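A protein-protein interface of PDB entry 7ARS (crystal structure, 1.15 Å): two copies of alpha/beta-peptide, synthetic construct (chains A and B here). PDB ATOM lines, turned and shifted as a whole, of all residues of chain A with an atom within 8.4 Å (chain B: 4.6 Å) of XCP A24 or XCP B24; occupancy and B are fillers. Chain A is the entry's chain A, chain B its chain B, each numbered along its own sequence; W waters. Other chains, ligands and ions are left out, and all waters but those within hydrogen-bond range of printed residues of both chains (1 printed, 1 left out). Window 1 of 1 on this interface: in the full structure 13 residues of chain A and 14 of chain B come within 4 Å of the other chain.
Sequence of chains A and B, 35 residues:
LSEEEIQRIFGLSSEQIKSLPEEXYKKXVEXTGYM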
ATOM      1  N   LEU A   1      -9.452  12.342   8.418  1.00  0.00           N
ATOM      2  CA  LEU A   1      -8.248  11.862   7.693  1.00  0.00           C
ATOM      3  C   LEU A   1      -8.602  10.503   7.108  1.00  0.00           C
ATOM      4  O   LEU A   1      -8.931   9.564   7.872  1.00  0.00           O
ATOM      5  CB  LEU A   1      -7.026  11.785   8.617  1.00  0.00           C
ATOM      6  CG  LEU A   1      -5.691  11.510   7.926  1.00  0.00           C
ATOM      7  CD1 LEU A   1      -5.342  12.604   6.933  1.00  0.00           C
ATOM      8  CD2 LEU A   1      -4.548  11.231   8.929  1.00  0.00           C
ATOM      9  N   GLU A   3      -8.096   7.058   4.413  1.00  0.00           N
ATOM     10  CA  GLU A   3      -7.036   6.222   3.818  1.00  0.00           C
ATOM     11  C   GLU A   3      -6.560   6.842   2.511  1.00  0.00           C
ATOM     12  O   GLU A   3      -5.366   6.810   2.246  1.00  0.00           O
ATOM     13  CB  GLU A   3      -7.441   4.743   3.675  1.00  0.00           C
ATOM     14  CG  GLU A   3      -8.081   4.147   4.916  1.00  0.00           C
ATOM     15  CD  GLU A   3      -8.459   2.693   4.757  1.00  0.00           C
ATOM     16  OE1 GLU A   3      -8.482   2.209   3.602  1.00  0.00           O
ATOM     17  OE2 GLU A   3      -8.791   2.048   5.776  1.00  0.00           O
ATOM     18  N   ILE A   6      -4.212   9.642   3.207  1.00  0.00           N
ATOM     19  CA  ILE A   6      -2.915   9.158   3.743  1.00  0.00           C
ATOM     20  C   ILE A   6      -2.081   8.599   2.588  1.00  0.00           C
ATOM     21  O   ILE A   6      -0.892   8.881   2.505  1.00  0.00           O
ATOM     22  CB  ILE A   6      -3.154   8.134   4.823  1.00  0.00           C
ATOM     23  CG1 ILE A   6      -3.686   8.828   6.060  1.00  0.00           C
ATOM     24  CG2 ILE A   6      -1.882   7.359   5.109  1.00  0.00           C
ATOM     25  CD1 ILE A   6      -4.376   7.911   7.001  1.00  0.00           C
ATOM     26  N   GLN A   7      -2.733   7.848   1.704  1.00  0.00           N
ATOM     27  CA  GLN A   7      -2.019   7.363   0.497  1.00  0.00           C
ATOM     28  C   GLN A   7      -1.349   8.488  -0.304  1.00  0.00           C
ATOM     29  O   GLN A   7      -0.176   8.380  -0.764  1.00  0.00           O
ATOM     30  CB  GLN A   7      -2.983   6.576  -0.377  1.00  0.00           C
ATOM     31  CG  GLN A   7      -2.306   6.178  -1.684  1.00  0.00           C
ATOM     32  CD  GLN A   7      -3.067   5.246  -2.570  1.00  0.00           C
ATOM     33  OE1 GLN A   7      -2.501   4.545  -3.397  1.00  0.00           O
ATOM     34  NE2 GLN A   7      -4.382   5.392  -2.578  1.00  0.00           N
ATOM     35  N   ILE A   9      -0.683  11.759   0.727  1.00  0.00           N
ATOM     36  CA  ILE A   9       0.300  12.473   1.571  1.00  0.00           C
ATOM     37  C   ILE A   9       1.661  11.734   1.521  1.00  0.00           C
ATOM     38  O   ILE A   9       2.705  12.350   1.480  1.00  0.00           O
ATOM     39  CB  ILE A   9      -0.232  12.634   2.994  1.00  0.00           C
ATOM     40  CG1 ILE A   9      -1.391  13.630   2.982  1.00  0.00           C
ATOM     41  CG2 ILE A   9       0.893  13.064   3.934  1.00  0.00           C
ATOM     42  CD1 ILE A   9      -2.219  13.622   4.234  1.00  0.00           C
ATOM     43  N   PHE A  10       1.679  10.418   1.642  1.00  0.00           N
ATOM     44  CA  PHE A  10       2.933   9.660   1.820  1.00  0.00           C
ATOM     45  C   PHE A  10       3.337   8.937   0.524  1.00  0.00           C
ATOM     46  O   PHE A  10       4.280   8.140   0.565  1.00  0.00           O
ATOM     47  CB  PHE A  10       2.759   8.692   2.978  1.00  0.00           C
ATOM     48  CG  PHE A  10       2.646   9.363   4.322  1.00  0.00           C
ATOM     49  CD1 PHE A  10       3.715  10.059   4.847  1.00  0.00           C
ATOM     50  CD2 PHE A  10       1.418   9.435   4.969  1.00  0.00           C
ATOM     51  CE1 PHE A  10       3.601  10.682   6.072  1.00  0.00           C
ATOM     52  CE2 PHE A  10       1.276  10.147   6.149  1.00  0.00           C
ATOM     53  CZ  PHE A  10       2.381  10.755   6.704  1.00  0.00           C
ATOM     54  N   LEU A  12       1.997   6.588  -1.307  1.00  0.00           N
ATOM     55  CA  LEU A  12       1.961   5.122  -1.108  1.00  0.00           C
ATOM     56  C   LEU A  12       1.445   4.446  -2.369  1.00  0.00           C
ATOM     57  O   LEU A  12       0.432   4.969  -2.994  1.00  0.00           O
ATOM     58  CB  LEU A  12       1.109   4.689   0.092  1.00  0.00           C
ATOM     59  CG  LEU A  12       1.558   5.231   1.439  1.00  0.00           C
ATOM     60  CD1 LEU A  12       0.627   4.801   2.544  1.00  0.00           C
ATOM     61  CD2 LEU A  12       2.993   4.797   1.733  1.00  0.00           C
ATOM     62  N   GLN A  16       1.341  -0.685  -0.934  1.00  0.00           N
ATOM     63  CA  GLN A  16       1.574  -0.217   0.422  1.00  0.00           C
ATOM     64  C   GLN A  16       0.286  -0.037   1.195  1.00  0.00           C
ATOM     65  O   GLN A  16       0.276  -0.199   2.421  1.00  0.00           O
ATOM     66  CB  GLN A  16       2.433   1.032   0.438  1.00  0.00           C
ATOM     67  CG  GLN A  16       3.880   0.764   0.040  1.00  0.00           C
ATOM     68  CD  GLN A  16       4.660   2.015  -0.219  1.00  0.00           C
ATOM     69  OE1 GLN A  16       4.146   2.980  -0.788  1.00  0.00           O
ATOM     70  NE2 GLN A  16       5.923   1.979   0.120  1.00  0.00           N
ATOM     71  N   ILE A  17      -0.790   0.417   0.544  1.00  0.00           N
ATOM     72  CA  ILE A  17      -2.044   0.701   1.300  1.00  0.00           C
ATOM     73  C   ILE A  17      -2.684  -0.600   1.774  1.00  0.00           C
ATOM     74  O   ILE A  17      -3.595  -0.514   2.617  1.00  0.00           O
ATOM     75  CB  ILE A  17      -3.037   1.549   0.497  1.00  0.00           C
ATOM     76  CG1 ILE A  17      -3.497   0.850  -0.778  1.00  0.00           C
ATOM     77  CG2 ILE A  17      -2.458   2.923   0.180  1.00  0.00           C
ATOM     78  CD1 ILE A  17      -4.601   1.568  -1.490  1.00  0.00           C
ATOM     79  N   SER A  19      -1.186  -2.462   3.707  1.00  0.00           N
ATOM     80  CA  SER A  19      -0.588  -2.522   5.049  1.00  0.00           C
ATOM     81  C   SER A  19      -0.468  -1.113   5.641  1.00  0.00           C
ATOM     82  O   SER A  19       0.633  -0.637   5.913  1.00  0.00           O
ATOM     83  CB  SER A  19       0.747  -3.252   5.042  1.00  0.00           C
ATOM     84  OG  SER A  19       0.620  -4.570   4.551  1.00  0.00           O
ATOM     85  N   LEU A  20      -1.605  -0.421   5.785  1.00  0.00           N
ATOM     86  CA  LEU A  20      -1.544   1.020   6.074  1.00  0.00           C
ATOM     87  C   LEU A  20      -0.882   1.292   7.414  1.00  0.00           C
ATOM     88  O   LEU A  20      -0.055   2.194   7.518  1.00  0.00           O
ATOM     89  CB  LEU A  20      -2.974   1.585   6.056  1.00  0.00           C
ATOM     90  CG  LEU A  20      -3.033   3.098   5.851  1.00  0.00           C
ATOM     91  CD1 LEU A  20      -2.573   3.439   4.446  1.00  0.00           C
ATOM     92  CD2 LEU A  20      -4.473   3.558   6.038  1.00  0.00           C
ATOM     93  N   PRO A  21      -1.175   0.526   8.495  1.00  0.00           N
ATOM     94  CA  PRO A  21      -0.504   0.878   9.747  1.00  0.00           C
ATOM     95  C   PRO A  21       1.018   0.708   9.694  1.00  0.00           C
ATOM     96  O   PRO A  21       1.755   1.523  10.294  1.00  0.00           O
ATOM     97  CB  PRO A  21      -1.143  -0.121  10.712  1.00  0.00           C
ATOM     98  CG  PRO A  21      -2.509  -0.376  10.129  1.00  0.00           C
ATOM     99  CD  PRO A  21      -2.241  -0.451   8.656  1.00  0.00           C
ATOM    100  N   GLU A  22       1.448  -0.333   8.965  1.00  0.00           N
ATOM    101  CA  GLU A  22       2.898  -0.606   8.858  1.00  0.00           C
ATOM    102  C   GLU A  22       3.637   0.366   7.947  1.00  0.00           C
ATOM    103  O   GLU A  22       4.758   0.725   8.233  1.00  0.00           O
ATOM    104  CB  GLU A  22       3.046  -2.042   8.373  1.00  0.00           C
ATOM    105  CG  GLU A  22       2.528  -3.117   9.273  1.00  0.00           C
ATOM    106  CD  GLU A  22       1.053  -3.467   9.175  1.00  0.00           C
ATOM    107  OE1 GLU A  22       0.277  -2.849   8.389  1.00  0.00           O
ATOM    108  OE2 GLU A  22       0.653  -4.415   9.825  1.00  0.00           O
ATOM    109  N   GLU A  23       2.984   0.688   6.843  1.00  0.00           N
ATOM    110  CA  GLU A  23       3.652   1.509   5.839  1.00  0.00           C
ATOM    111  C   GLU A  23       3.564   3.017   6.179  1.00  0.00           C
ATOM    112  O   GLU A  23       4.534   3.730   5.952  1.00  0.00           O
ATOM    113  CB  GLU A  23       3.034   1.213   4.466  1.00  0.00           C
ATOM    114  CG  GLU A  23       3.333  -0.202   4.026  1.00  0.00           C
ATOM    115  CD  GLU A  23       4.751  -0.470   3.656  1.00  0.00           C
ATOM    116  OE1 GLU A  23       5.491   0.398   3.288  1.00  0.00           O
ATOM    117  OE2 GLU A  23       5.131  -1.677   3.801  1.00  0.00           O
ATOM    118  N   XCP A  24       2.454   3.402   6.813  1.00  0.00           N
ATOM    119  CB  XCP A  24       2.328   4.772   7.296  1.00  0.00           C
ATOM    120  CG  XCP A  24       1.035   5.443   6.792  1.00  0.00           C
ATOM    121  CD  XCP A  24       0.901   6.651   7.692  1.00  0.00           C
ATOM    122  CE  XCP A  24       1.368   6.098   9.054  1.00  0.00           C
ATOM    123  CA  XCP A  24       2.101   4.786   8.816  1.00  0.00           C
ATOM    124  C   XCP A  24       3.497   4.729   9.480  1.00  0.00           C
ATOM    125  O   XCP A  24       4.230   5.683   9.565  1.00  0.00           O
ATOM    126  N   TYR A  25       3.751   3.518  10.113  1.00  0.00           N
ATOM    127  CA  TYR A  25       5.016   3.368  10.883  1.00  0.00           C
ATOM    128  C   TYR A  25       6.241   3.796  10.093  1.00  0.00           C
ATOM    129  O   TYR A  25       7.063   4.562  10.583  1.00  0.00           O
ATOM    130  CB  TYR A  25       5.111   1.918  11.375  1.00  0.00           C
ATOM    131  CG  TYR A  25       6.236   1.668  12.348  1.00  0.00           C
ATOM    132  CD1 TYR A  25       7.537   1.590  11.918  1.00  0.00           C
ATOM    133  CD2 TYR A  25       5.946   1.602  13.693  1.00  0.00           C
ATOM    134  CE1 TYR A  25       8.559   1.357  12.864  1.00  0.00           C
ATOM    135  CE2 TYR A  25       6.974   1.348  14.620  1.00  0.00           C
ATOM    136  CZ  TYR A  25       8.274   1.308  14.195  1.00  0.00           C
ATOM    137  OH  TYR A  25       9.343   1.135  15.049  1.00  0.00           O
ATOM    138  N   LYS A  26       6.398   3.252   8.913  1.00  0.00           N
ATOM    139  CA  LYS A  26       7.638   3.482   8.125  1.00  0.00           C
ATOM    140  C   LYS A  26       7.728   4.941   7.638  1.00  0.00           C
ATOM    141  O   LYS A  26       8.773   5.565   7.770  1.00  0.00           O
ATOM    142  CB  LYS A  26       7.755   2.604   6.921  1.00  0.00           C
ATOM    143  CG  LYS A  26       8.029   1.125   7.256  1.00  0.00           C
ATOM    144  CD  LYS A  26       7.946   0.255   5.959  1.00  0.00           C
ATOM    145  CE  LYS A  26       8.023  -1.223   6.098  1.00  0.00           C
ATOM    146  NZ  LYS A  26       7.962  -1.834   4.739  1.00  0.00           N
ATOM    147  N   LYS A  27       6.656   5.484   7.051  1.00  0.00           N
ATOM    148  CA  LYS A  27       6.689   6.876   6.574  1.00  0.00           C
ATOM    149  C   LYS A  27       6.782   7.815   7.743  1.00  0.00           C
ATOM    150  O   LYS A  27       7.457   8.947   7.468  1.00  0.00           O
ATOM    151  CB  LYS A  27       5.459   7.191   5.730  1.00  0.00           C
ATOM    152  CG  LYS A  27       5.495   6.495   4.401  1.00  0.00           C
ATOM    153  CD  LYS A  27       6.465   6.997   3.394  1.00  0.00           C
ATOM    154  CE  LYS A  27       6.296   6.291   2.056  1.00  0.00           C
ATOM    155  NZ  LYS A  27       6.737   7.123   0.919  1.00  0.00           N
ATOM    156  N   XCP A  28       6.191   7.600   8.875  1.00  0.00           N
ATOM    157  CB  XCP A  28       6.200   8.479   9.983  1.00  0.00           C
ATOM    158  CG  XCP A  28       4.853   9.067  10.324  1.00  0.00           C
ATOM    159  CD  XCP A  28       5.078   9.636  11.744  1.00  0.00           C
ATOM    160  CE  XCP A  28       6.026   8.603  12.400  1.00  0.00           C
ATOM    161  CA  XCP A  28       6.651   7.795  11.267  1.00  0.00           C
ATOM    162  C   XCP A  28       8.197   7.845  11.356  1.00  0.00           C
ATOM    163  O   XCP A  28       8.818   8.793  11.712  1.00  0.00           O
ATOM    164  N   VAL A  29       8.875   6.700  10.935  1.00  0.00           N
ATOM    165  CA  VAL A  29      10.325   6.652  11.001  1.00  0.00           C
ATOM    166  C   VAL A  29      10.948   7.741  10.148  1.00  0.00           C
ATOM    167  O   VAL A  29      11.802   8.469  10.615  1.00  0.00           O
ATOM    168  CB  VAL A  29      10.786   5.239  10.587  1.00  0.00           C
ATOM    169  CG1 VAL A  29      12.288   5.256  10.504  1.00  0.00           C
ATOM    170  CG2 VAL A  29      10.280   4.177  11.560  1.00  0.00           C
ATOM    171  N   GLU A  30      10.548   7.783   8.860  1.00  0.00           N
ATOM    172  CA  GLU A  30      11.223   8.691   7.925  1.00  0.00           C
ATOM    173  C   GLU A  30      10.942  10.137   8.349  1.00  0.00           C
ATOM    174  O   GLU A  30      11.856  10.931   8.468  1.00  0.00           O
ATOM    175  CB  GLU A  30      10.700   8.426   6.516  1.00  0.00           C
ATOM    176  CG  GLU A  30      11.419   9.293   5.446  1.00  0.00           C
ATOM    177  CD  GLU A  30      11.127   8.986   4.007  1.00  0.00           C
ATOM    178  OE1 GLU A  30      10.215   8.277   3.719  1.00  0.00           O
ATOM    179  OE2 GLU A  30      11.722   9.690   3.164  1.00  0.00           O
ATOM    180  N   XCP A  31       9.673  10.503   8.484  1.00  0.00           N
ATOM    181  CB  XCP A  31       9.292  11.863   8.939  1.00  0.00           C
ATOM    182  CG  XCP A  31       8.025  12.374   8.144  1.00  0.00           C
ATOM    183  CD  XCP A  31       6.955  12.574   9.238  1.00  0.00           C
ATOM    184  CE  XCP A  31       7.797  12.946  10.488  1.00  0.00           C
ATOM    185  CA  XCP A  31       8.895  11.897  10.460  1.00  0.00           C
ATOM    186  C   XCP A  31      10.111  12.210  11.285  1.00  0.00           C
ATOM    187  O   XCP A  31      10.652  13.286  11.373  1.00  0.00           O
ATOM    188  N   ILE B   6       3.013  16.187  11.615  1.00  0.00           N
ATOM    189  CA  ILE B   6       2.377  14.861  11.758  1.00  0.00           C
ATOM    190  C   ILE B   6       1.401  14.918  12.941  1.00  0.00           C
ATOM    191  O   ILE B   6       0.274  14.443  12.859  1.00  0.00           O
ATOM    192  CB  ILE B   6       3.444  13.765  12.006  1.00  0.00           C
ATOM    193  CG1 ILE B   6       4.278  13.556  10.747  1.00  0.00           C
ATOM    194  CG2 ILE B   6       2.824  12.441  12.475  1.00  0.00           C
ATOM    195  CD1 ILE B   6       3.526  12.881   9.585  1.00  0.00           C
ATOM    196  N   PHE B  10      -2.561  14.138  12.089  1.00  0.00           N
ATOM    197  CA  PHE B  10      -3.115  12.910  12.739  1.00  0.00           C
ATOM    198  C   PHE B  10      -3.864  13.254  14.031  1.00  0.00           C
ATOM    199  O   PHE B  10      -4.489  12.319  14.573  1.00  0.00           O
ATOM    200  CB  PHE B  10      -2.060  11.815  12.972  1.00  0.00           C
ATOM    201  CG  PHE B  10      -1.581  11.213  11.680  1.00  0.00           C
ATOM    202  CD1 PHE B  10      -0.616  11.833  10.927  1.00  0.00           C
ATOM    203  CD2 PHE B  10      -2.132  10.047  11.169  1.00  0.00           C
ATOM    204  CE1 PHE B  10      -0.142  11.285   9.741  1.00  0.00           C
ATOM    205  CE2 PHE B  10      -1.651   9.490   9.995  1.00  0.00           C
ATOM    206  CZ  PHE B  10      -0.636  10.089   9.301  1.00  0.00           C
ATOM    207  N   LEU B  12      -2.689  14.270  17.208  1.00  0.00           N
ATOM    208  CA  LEU B  12      -2.018  13.539  18.312  1.00  0.00           C
ATOM    209  C   LEU B  12      -1.933  14.383  19.592  1.00  0.00           C
ATOM    210  O   LEU B  12      -1.318  15.475  19.566  1.00  0.00           O
ATOM    211  CB  LEU B  12      -0.624  13.067  17.866  1.00  0.00           C
ATOM    212  CG  LEU B  12      -0.584  12.248  16.583  1.00  0.00           C
ATOM    213  CD1 LEU B  12       0.823  11.842  16.243  1.00  0.00           C
ATOM    214  CD2 LEU B  12      -1.499  11.061  16.696  1.00  0.00           C
ATOM    215  N   LEU B  20       6.913   8.241  18.094  1.00  0.00           N
ATOM    216  CA  LEU B  20       6.027   8.663  17.014  1.00  0.00           C
ATOM    217  C   LEU B  20       5.697   7.567  16.019  1.00  0.00           C
ATOM    218  O   LEU B  20       4.544   7.408  15.646  1.00  0.00           O
ATOM    219  CB  LEU B  20       6.629   9.918  16.331  1.00  0.00           C
ATOM    220  CG  LEU B  20       5.655  10.673  15.448  1.00  0.00           C
ATOM    221  CD1 LEU B  20       4.499  11.313  16.232  1.00  0.00           C
ATOM    222  CD2 LEU B  20       6.437  11.686  14.615  1.00  0.00           C
ATOM    223  N   PRO B  21       6.684   6.711  15.640  1.00  0.00           N
ATOM    224  CA  PRO B  21       6.332   5.651  14.722  1.00  0.00           C
ATOM    225  C   PRO B  21       5.264   4.723  15.281  1.00  0.00           C
ATOM    226  O   PRO B  21       4.375   4.298  14.565  1.00  0.00           O
ATOM    227  CB  PRO B  21       7.674   4.932  14.426  1.00  0.00           C
ATOM    228  CG  PRO B  21       8.688   6.084  14.631  1.00  0.00           C
ATOM    229  CD  PRO B  21       8.161   6.813  15.815  1.00  0.00           C
ATOM    230  N   GLU B  22       5.398   4.354  16.559  1.00  0.00           N
ATOM    231  CA  GLU B  22       4.412   3.466  17.184  1.00  0.00           C
ATOM    232  C   GLU B  22       3.032   4.085  17.352  1.00  0.00           C
ATOM    233  O   GLU B  22       2.025   3.484  17.094  1.00  0.00           O
ATOM    234  CB  GLU B  22       4.926   2.950  18.538  1.00  0.00           C
ATOM    235  CG  GLU B  22       6.162   2.092  18.440  1.00  0.00           C
ATOM    236  CD  GLU B  22       6.722   1.643  19.780  1.00  0.00           C
ATOM    237  OE1 GLU B  22       6.155   2.032  20.821  1.00  0.00           O
ATOM    238  OE2 GLU B  22       7.811   0.993  19.794  1.00  0.00           O
ATOM    239  N   GLU B  23       3.035   5.297  17.851  1.00  0.00           N
ATOM    240  CA  GLU B  23       1.790   5.976  18.210  1.00  0.00           C
ATOM    241  C   GLU B  23       1.027   6.479  16.981  1.00  0.00           C
ATOM    242  O   GLU B  23      -0.208   6.386  16.974  1.00  0.00           O
ATOM    243  CB  GLU B  23       2.073   7.054  19.240  1.00  0.00           C
ATOM    244  CG  GLU B  23       2.465   6.490  20.618  1.00  0.00           C
ATOM    245  CD  GLU B  23       1.543   5.485  21.283  1.00  0.00           C
ATOM    246  OE1 GLU B  23       0.286   5.683  21.275  1.00  0.00           O
ATOM    247  OE2 GLU B  23       2.003   4.415  21.739  1.00  0.00           O
ATOM    248  N   XCP B  24       1.759   6.858  15.978  1.00  0.00           N
ATOM    249  CB  XCP B  24       1.188   7.368  14.706  1.00  0.00           C
ATOM    250  CG  XCP B  24       1.580   8.802  14.405  1.00  0.00           C
ATOM    251  CD  XCP B  24       1.251   8.858  12.957  1.00  0.00           C
ATOM    252  CE  XCP B  24       1.555   7.554  12.380  1.00  0.00           C
ATOM    253  CA  XCP B  24       1.739   6.569  13.520  1.00  0.00           C
ATOM    254  C   XCP B  24       0.983   5.299  13.332  1.00  0.00           C
ATOM    255  O   XCP B  24      -0.223   5.236  12.928  1.00  0.00           O
ATOM    256  N   TYR B  25       1.563   4.110  13.757  1.00  0.00           N
ATOM    257  CA  TYR B  25       0.949   2.814  13.571  1.00  0.00           C
ATOM    258  C   TYR B  25      -0.420   2.734  14.271  1.00  0.00           C
ATOM    259  O   TYR B  25      -1.372   2.263  13.625  1.00  0.00           O
ATOM    260  CB  TYR B  25       1.915   1.750  14.125  1.00  0.00           C
ATOM    261  CG  TYR B  25       1.386   0.331  14.124  1.00  0.00           C
ATOM    262  CD1 TYR B  25       0.576  -0.186  15.112  1.00  0.00           C
ATOM    263  CD2 TYR B  25       1.610  -0.444  13.032  1.00  0.00           C
ATOM    264  CE1 TYR B  25       0.056  -1.481  15.060  1.00  0.00           C
ATOM    265  CE2 TYR B  25       1.139  -1.737  12.943  1.00  0.00           C
ATOM    266  CZ  TYR B  25       0.308  -2.237  13.937  1.00  0.00           C
ATOM    267  OH  TYR B  25      -0.185  -3.507  13.880  1.00  0.00           O
ATOM    268  N   LYS B  26      -0.523   3.149  15.511  1.00  0.00           N
ATOM    269  CA  LYS B  26      -1.790   2.970  16.272  1.00  0.00           C
ATOM    270  C   LYS B  26      -2.835   3.934  15.748  1.00  0.00           C
ATOM    271  O   LYS B  26      -3.985   3.531  15.479  1.00  0.00           O
ATOM    272  CB  LYS B  26      -1.618   3.218  17.749  1.00  0.00           C
ATOM    273  CG  LYS B  26      -0.785   2.126  18.403  1.00  0.00           C
ATOM    274  CD  LYS B  26      -0.569   2.421  19.864  1.00  0.00           C
ATOM    275  CE  LYS B  26       0.481   1.525  20.458  1.00  0.00           C
ATOM    276  NZ  LYS B  26       0.714   1.873  21.880  1.00  0.00           N
ATOM    277  N   LYS B  27      -2.530   5.222  15.573  1.00  0.00           N
ATOM    278  CA  LYS B  27      -3.563   6.184  15.091  1.00  0.00           C
ATOM    279  C   LYS B  27      -3.940   5.837  13.667  1.00  0.00           C
ATOM    280  O   LYS B  27      -5.173   6.134  13.325  1.00  0.00           O
ATOM    281  CB  LYS B  27      -3.024   7.605  15.189  1.00  0.00           C
ATOM    282  CG  LYS B  27      -2.953   8.098  16.623  1.00  0.00           C
ATOM    283  CD  LYS B  27      -4.310   8.501  17.159  1.00  0.00           C
ATOM    284  CE  LYS B  27      -4.191   9.194  18.504  1.00  0.00           C
ATOM    285  NZ  LYS B  27      -5.498   9.699  18.979  1.00  0.00           N
ATOM    286  N   XCP B  28      -3.071   5.425  12.843  1.00  0.00           N
ATOM    287  CB  XCP B  28      -3.306   5.120  11.461  1.00  0.00           C
ATOM    288  CG  XCP B  28      -2.598   5.954  10.468  1.00  0.00           C
ATOM    289  CD  XCP B  28      -2.661   5.143   9.210  1.00  0.00           C
ATOM    290  CE  XCP B  28      -2.744   3.721   9.571  1.00  0.00           C
ATOM    291  CA  XCP B  28      -2.989   3.665  11.078  1.00  0.00           C
ATOM    292  C   XCP B  28      -4.075   2.738  11.421  1.00  0.00           C
ATOM    293  O   XCP B  28      -5.093   2.633  10.708  1.00  0.00           O
HETATM  294  O   HOH W   1       8.953   0.328  17.526  1.00  0.00           O
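Of the 12 printed residues of chain B, 8 touch a printed residue of chain A.
Printed residues of chain B that touch a printed residue of chain A: Ile B6, Phe B10, Leu B20, Pro B21, Glu B22, XCP B24, Tyr B25 and XCP B28.
Hydrophobic or aromatic side chains of chain B within 4 Å of the printed part of chain A: Ile B6, Phe B10, Leu B20, Pro B21 and Tyr B25.
Printed residues of chain A that touch a printed residue of chain B: Leu A1, Ile A6, Phe A10, Leu A20, Pro A21, XCP A24, Tyr A25, XCP A28, Val A29 and XCP A31.
Along chain A the printed residues that touch a printed residue of chain B span positions 1 to 31.
Among the printed residues, 15 pairs touch across the chains.
Among the printed residues, no Asp or Glu carboxylate lies within 4 Å of a Lys or Arg side-chain nitrogen of the other chain.
Leu A1 touches Phe B10 (CD2 to CD2, 3.5 Å).
Ile B6 touches Phe A10 (CD1 to CZ, 3.8 Å).
CE of XCP B28 touches O of Leu A20, at 3.7 Å.
Pro A21 touches XCP B28 (CA to CE, 3.6 Å).
XCP B24 touches XCP A24 (CE to CE, 3.6 Å).
Tyr A25 touches Pro B21 (CD2 to O, 3.2 Å).
CG2 of Ile B6 touches CD of XCP A28, 3.7 Å away.
CE of XCP A28 touches CG of Leu B20 (3.7 Å).
Pro B21 touches Val A29.
XCP A31 touches Ile B6 (CD to CG1, 3.2 Å).
Of chain B, only XCP B24 (3.6 Å) comes within 4 Å of XCP A24.
XCP B24 touches just one residue of chain A: XCP A24.
Of the printed residues of chain B, Val A29 touches Pro B21.
Printed residues of chain B within 4 Å of Leu A20: XCP B28 (3.7 Å).
The nearest printed residue of chain B that does not touch XCP A24 is Phe B10 (4.1 Å).
The nearest residue of chain A that does not touch XCP B24 is XCP A28 (4.1 Å).
The nearest printed residue of chain B that does not touch Tyr A25 is Tyr B25 (4.1 Å).
The backbone carbonyl oxygen (O) of Phe A10 lies within hydrogen-bond range of the side-chain amino group (NZ) of Lys A27, 2.7 Å away.
Water W1 lies within hydrogen-bond range of OE2 of Glu B22 and OH of Tyr A25.
Phe A10 touches Ile B6, but with the chains exchanged Ile A6 does not touch Phe B10 (4.3 Å).
Phe B10 touches its own counterpart, Phe A10.
XCP A24 touches its own counterpart, XCP B24.
Tyr A25 touches Glu B22, but with the chains exchanged Glu A22 does not touch Tyr B25 (4.1 Å).
Positions printed for both chains: 6, 10, 12, 20, 21, 22, 23, 24, 25, 26, 27 and 28.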
